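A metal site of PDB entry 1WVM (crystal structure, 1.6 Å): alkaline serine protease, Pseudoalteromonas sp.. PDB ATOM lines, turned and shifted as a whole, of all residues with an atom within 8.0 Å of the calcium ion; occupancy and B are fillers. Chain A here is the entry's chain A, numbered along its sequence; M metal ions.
OE1 of Glu 2 lies close to N of Asn 79, 3.4 Å away.
Of the 21 residues printed, 6 come within 4 Å of the calcium ion.
O of Glu 80 is bound to the calcium ion, 2.3 Å away.
O of Ile 76 binds the calcium ion (2.3 Å).
OE1 of Glu 2 binds the calcium ion.
The backbone carbonyl oxygen (O) of Val 82 binds the calcium ion, at 2.4 Å.
The calcium ion is bound by the side-chain amide oxygen (OD1) of Asn 78, at 2.4 Å.
The calcium ion is bound by OD1 of Asp 39, at 2.4 Å.
OD2 of Asp 39 is bound to the calcium ion (2.6 Å).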
ATOM      1  N   ALA A   1       5.372 -10.884 -11.021  1.00  0.00           N
ATOM      2  CA  ALA A   1       4.183 -10.403 -11.776  1.00  0.00           C
ATOM      3  C   ALA A   1       3.444 -11.574 -12.403  1.00  0.00           C
ATOM      4  O   ALA A   1       4.062 -12.517 -12.902  1.00  0.00           O
ATOM      5  CB  ALA A   1       4.623  -9.421 -12.853  1.00  0.00           C
ATOM      6  N   GLU A   2       2.130 -11.500 -12.380  1.00  0.00           N
ATOM      7  CA  GLU A   2       1.286 -12.555 -12.939  1.00  0.00           C
ATOM      8  C   GLU A   2       0.519 -12.025 -14.137  1.00  0.00           C
ATOM      9  O   GLU A   2      -0.076 -10.949 -14.085  1.00  0.00           O
ATOM     10  CB  GLU A   2       0.322 -13.052 -11.860  1.00  0.00           C
ATOM     11  CG  GLU A   2      -0.610 -14.149 -12.287  1.00  0.00           C
ATOM     12  CD  GLU A   2      -1.298 -14.751 -11.084  1.00  0.00           C
ATOM     13  OE1 GLU A   2      -0.872 -15.836 -10.641  1.00  0.00           O
ATOM     14  OE2 GLU A   2      -2.242 -14.124 -10.562  1.00  0.00           O
ATOM     15  N   THR A   3       0.529 -12.797 -15.217  1.00  0.00           N
ATOM     16  CA  THR A   3      -0.144 -12.407 -16.449  1.00  0.00           C
ATOM     17  C   THR A   3      -1.420 -13.205 -16.673  1.00  0.00           C
ATOM     18  O   THR A   3      -1.487 -14.400 -16.379  1.00  0.00           O
ATOM     19  CB  THR A   3       0.788 -12.606 -17.663  1.00  0.00           C
ATOM     20  OG1 THR A   3       1.952 -11.767 -17.520  1.00  0.00           O
ATOM     21  CG2 THR A   3       0.079 -12.250 -18.955  1.00  0.00           C
ATOM     22  N   HIS A  37       5.727 -27.820 -10.637  1.00  0.00           N
ATOM     23  CA  HIS A  37       5.572 -26.444 -11.118  1.00  0.00           C
ATOM     24  C   HIS A  37       4.929 -25.533 -10.073  1.00  0.00           C
ATOM     25  O   HIS A  37       3.920 -25.897  -9.473  1.00  0.00           O
ATOM     26  CB  HIS A  37       4.719 -26.437 -12.400  1.00  0.00           C
ATOM     27  CG  HIS A  37       4.766 -25.148 -13.138  1.00  0.00           C
ATOM     28  ND1 HIS A  37       5.263 -25.047 -14.426  1.00  0.00           N
ATOM     29  CD2 HIS A  37       4.397 -23.893 -12.779  1.00  0.00           C
ATOM     30  CE1 HIS A  37       5.201 -23.775 -14.814  1.00  0.00           C
ATOM     31  NE2 HIS A  37       4.682 -23.070 -13.833  1.00  0.00           N
ATOM     32  N   ASN A  38       5.499 -24.353  -9.873  1.00  0.00           N
ATOM     33  CA  ASN A  38       4.970 -23.407  -8.891  1.00  0.00           C
ATOM     34  C   ASN A  38       3.526 -22.981  -9.112  1.00  0.00           C
ATOM     35  O   ASN A  38       2.819 -22.634  -8.157  1.00  0.00           O
ATOM     36  CB  ASN A  38       5.850 -22.158  -8.833  1.00  0.00           C
ATOM     37  CG  ASN A  38       7.277 -22.461  -8.426  1.00  0.00           C
ATOM     38  OD1 ASN A  38       7.524 -23.245  -7.503  1.00  0.00           O
ATOM     39  ND2 ASN A  38       8.234 -21.848  -9.117  1.00  0.00           N
ATOM     40  N   ASP A  39       3.065 -22.998 -10.353  1.00  0.00           N
ATOM     41  CA  ASP A  39       1.696 -22.591 -10.651  1.00  0.00           C
ATOM     42  C   ASP A  39       0.725 -23.771 -10.667  1.00  0.00           C
ATOM     43  O   ASP A  39      -0.463 -23.601 -10.950  1.00  0.00           O
ATOM     44  CB  ASP A  39       1.630 -21.848 -11.994  1.00  0.00           C
ATOM     45  CG  ASP A  39       1.399 -20.361 -11.836  1.00  0.00           C
ATOM     46  OD1 ASP A  39       1.600 -19.826 -10.724  1.00  0.00           O
ATOM     47  OD2 ASP A  39       1.003 -19.706 -12.826  1.00  0.00           O
ATOM     48  N   LEU A  40       1.217 -24.966 -10.321  1.00  0.00           N
ATOM     49  CA  LEU A  40       0.380 -26.161 -10.322  1.00  0.00           C
ATOM     50  C   LEU A  40       0.521 -27.056  -9.086  1.00  0.00           C
ATOM     51  O   LEU A  40      -0.374 -27.849  -8.779  1.00  0.00           O
ATOM     52  CB  LEU A  40       0.683 -27.019 -11.562  1.00  0.00           C
ATOM     53  CG  LEU A  40       0.403 -26.408 -12.939  1.00  0.00           C
ATOM     54  CD1 LEU A  40       0.915 -27.365 -14.026  1.00  0.00           C
ATOM     55  CD2 LEU A  40      -1.094 -26.153 -13.096  1.00  0.00           C
ATOM     56  N   ALA A  74      -6.370 -24.593 -14.476  1.00  0.00           N
ATOM     57  CA  ALA A  74      -6.169 -24.203 -13.089  1.00  0.00           C
ATOM     58  C   ALA A  74      -4.829 -23.630 -12.652  1.00  0.00           C
ATOM     59  O   ALA A  74      -4.407 -23.859 -11.513  1.00  0.00           O
ATOM     60  CB  ALA A  74      -6.524 -25.383 -12.209  1.00  0.00           C
ATOM     61  N   ALA A  75      -4.145 -22.894 -13.523  1.00  0.00           N
ATOM     62  CA  ALA A  75      -2.881 -22.287 -13.107  1.00  0.00           C
ATOM     63  C   ALA A  75      -3.253 -21.430 -11.900  1.00  0.00           C
ATOM     64  O   ALA A  75      -4.231 -20.686 -11.923  1.00  0.00           O
ATOM     65  CB  ALA A  75      -2.310 -21.420 -14.228  1.00  0.00           C
ATOM     66  N   ILE A  76      -2.465 -21.549 -10.831  1.00  0.00           N
ATOM     67  CA  ILE A  76      -2.745 -20.862  -9.576  1.00  0.00           C
ATOM     68  C   ILE A  76      -2.503 -19.348  -9.555  1.00  0.00           C
ATOM     69  O   ILE A  76      -1.507 -18.862 -10.083  1.00  0.00           O
ATOM     70  CB  ILE A  76      -1.955 -21.517  -8.426  1.00  0.00           C
ATOM     71  CG1 ILE A  76      -2.380 -22.979  -8.293  1.00  0.00           C
ATOM     72  CG2 ILE A  76      -2.183 -20.763  -7.117  1.00  0.00           C
ATOM     73  CD1 ILE A  76      -1.488 -23.796  -7.378  1.00  0.00           C
ATOM     74  N   ALA A  77      -3.437 -18.620  -8.941  1.00  0.00           N
ATOM     75  CA  ALA A  77      -3.329 -17.171  -8.801  1.00  0.00           C
ATOM     76  C   ALA A  77      -2.367 -16.950  -7.641  1.00  0.00           C
ATOM     77  O   ALA A  77      -2.665 -17.320  -6.504  1.00  0.00           O
ATOM     78  CB  ALA A  77      -4.697 -16.564  -8.491  1.00  0.00           C
ATOM     79  N   ASN A  78      -1.220 -16.337  -7.925  1.00  0.00           N
ATOM     80  CA  ASN A  78      -0.197 -16.133  -6.907  1.00  0.00           C
ATOM     81  C   ASN A  78       0.860 -15.073  -7.232  1.00  0.00           C
ATOM     82  O   ASN A  78       1.986 -15.158  -6.752  1.00  0.00           O
ATOM     83  CB  ASN A  78       0.516 -17.450  -6.650  1.00  0.00           C
ATOM     84  CG  ASN A  78       0.990 -18.112  -7.942  1.00  0.00           C
ATOM     85  OD1 ASN A  78       1.140 -17.442  -8.969  1.00  0.00           O
ATOM     86  ND2 ASN A  78       1.230 -19.414  -7.893  1.00  0.00           N
ATOM     87  N   ASN A  79       0.519 -14.089  -8.054  1.00  0.00           N
ATOM     88  CA  ASN A  79       1.476 -13.033  -8.406  1.00  0.00           C
ATOM     89  C   ASN A  79       2.708 -13.515  -9.198  1.00  0.00           C
ATOM     90  O   ASN A  79       3.761 -12.872  -9.160  1.00  0.00           O
ATOM     91  CB  ASN A  79       1.959 -12.310  -7.137  1.00  0.00           C
ATOM     92  CG  ASN A  79       2.719 -11.025  -7.443  1.00  0.00           C
ATOM     93  OD1 ASN A  79       3.691 -10.684  -6.770  1.00  0.00           O
ATOM     94  ND2 ASN A  79       2.261 -10.304  -8.459  1.00  0.00           N
ATOM     95  N   GLU A  80       2.595 -14.643  -9.888  1.00  0.00           N
ATOM     96  CA  GLU A  80       3.700 -15.137 -10.718  1.00  0.00           C
ATOM     97  C   GLU A  80       3.094 -16.011 -11.804  1.00  0.00           C
ATOM     98  O   GLU A  80       1.995 -16.535 -11.649  1.00  0.00           O
ATOM     99  CB  GLU A  80       4.704 -15.948  -9.891  1.00  0.00           C
ATOM    100  CG  GLU A  80       4.485 -17.461  -9.846  1.00  0.00           C
ATOM    101  CD  GLU A  80       5.517 -18.176  -8.996  1.00  0.00           C
ATOM    102  OE1 GLU A  80       5.493 -18.006  -7.759  1.00  0.00           O
ATOM    103  OE2 GLU A  80       6.364 -18.906  -9.561  1.00  0.00           O
ATOM    104  N   GLY A  81       3.796 -16.143 -12.927  1.00  0.00           N
ATOM    105  CA  GLY A  81       3.281 -16.958 -14.012  1.00  0.00           C
ATOM    106  C   GLY A  81       1.957 -16.471 -14.583  1.00  0.00           C
ATOM    107  O   GLY A  81       1.822 -15.301 -14.946  1.00  0.00           O
ATOM    108  N   VAL A  82       0.986 -17.376 -14.667  1.00  0.00           N
ATOM    109  CA  VAL A  82      -0.332 -17.028 -15.213  1.00  0.00           C
ATOM    110  C   VAL A  82      -1.442 -17.487 -14.283  1.00  0.00           C
ATOM    111  O   VAL A  82      -1.200 -17.803 -13.111  1.00  0.00           O
ATOM    112  CB  VAL A  82      -0.536 -17.693 -16.606  1.00  0.00           C
ATOM    113  CG1 VAL A  82       0.541 -17.207 -17.569  1.00  0.00           C
ATOM    114  CG2 VAL A  82      -0.477 -19.204 -16.473  1.00  0.00           C
ATOM    115  N   VAL A  83      -2.675 -17.497 -14.810  1.00  0.00           N
ATOM    116  CA  VAL A  83      -3.851 -17.935 -14.063  1.00  0.00           C
ATOM    117  C   VAL A  83      -4.736 -18.742 -14.992  1.00  0.00           C
ATOM    118  O   VAL A  83      -4.826 -18.447 -16.186  1.00  0.00           O
ATOM    119  CB  VAL A  83      -4.675 -16.729 -13.507  1.00  0.00           C
ATOM    120  CG1 VAL A  83      -3.873 -15.978 -12.463  1.00  0.00           C
ATOM    121  CG2 VAL A  83      -5.072 -15.797 -14.639  1.00  0.00           C
ATOM    122  N   GLY A  84      -5.383 -19.769 -14.439  1.00  0.00           N
ATOM    123  CA  GLY A  84      -6.268 -20.608 -15.215  1.00  0.00           C
ATOM    124  C   GLY A  84      -7.717 -20.219 -14.958  1.00  0.00           C
ATOM    125  O   GLY A  84      -7.974 -19.269 -14.213  1.00  0.00           O
ATOM    126  N   PRO A  87      -8.385 -20.553 -10.750  1.00  0.00           N
ATOM    127  CA  PRO A  87      -7.068 -20.354 -10.131  1.00  0.00           C
ATOM    128  C   PRO A  87      -6.916 -20.287  -8.619  1.00  0.00           C
ATOM    129  O   PRO A  87      -5.784 -20.159  -8.138  1.00  0.00           O
ATOM    130  CB  PRO A  87      -6.625 -19.049 -10.765  1.00  0.00           C
ATOM    131  CG  PRO A  87      -7.906 -18.252 -10.665  1.00  0.00           C
ATOM    132  CD  PRO A  87      -8.991 -19.260 -11.087  1.00  0.00           C
ATOM    133  N   THR A 208       1.292 -22.925 -18.546  1.00  0.00           N
ATOM    134  CA  THR A 208       2.378 -23.613 -17.860  1.00  0.00           C
ATOM    135  C   THR A 208       2.870 -24.813 -18.671  1.00  0.00           C
ATOM    136  O   THR A 208       2.098 -25.452 -19.373  1.00  0.00           O
ATOM    137  CB  THR A 208       1.886 -24.151 -16.516  1.00  0.00           C
ATOM    138  OG1 THR A 208       0.684 -24.921 -16.724  1.00  0.00           O
ATOM    139  CG2 THR A 208       1.585 -23.012 -15.554  1.00  0.00           C
ATOM    140  N   TYR A 362       6.859 -21.540 -18.888  1.00  0.00           N
ATOM    141  CA  TYR A 362       5.596 -21.231 -19.571  1.00  0.00           C
ATOM    142  C   TYR A 362       5.907 -21.166 -21.059  1.00  0.00           C
ATOM    143  O   TYR A 362       7.055 -20.991 -21.443  1.00  0.00           O
ATOM    144  CB  TYR A 362       5.069 -19.871 -19.108  1.00  0.00           C
ATOM    145  CG  TYR A 362       4.908 -19.770 -17.616  1.00  0.00           C
ATOM    146  CD1 TYR A 362       3.720 -20.181 -16.993  1.00  0.00           C
ATOM    147  CD2 TYR A 362       5.964 -19.366 -16.809  1.00  0.00           C
ATOM    148  CE1 TYR A 362       3.603 -20.178 -15.614  1.00  0.00           C
ATOM    149  CE2 TYR A 362       5.856 -19.361 -15.430  1.00  0.00           C
ATOM    150  CZ  TYR A 362       4.672 -19.769 -14.838  1.00  0.00           C
ATOM    151  OH  TYR A 362       4.568 -19.776 -13.466  1.00  0.00           O
HETATM  152 CA    CA M   1       0.217 -17.864 -11.179  1.00  0.00          CA
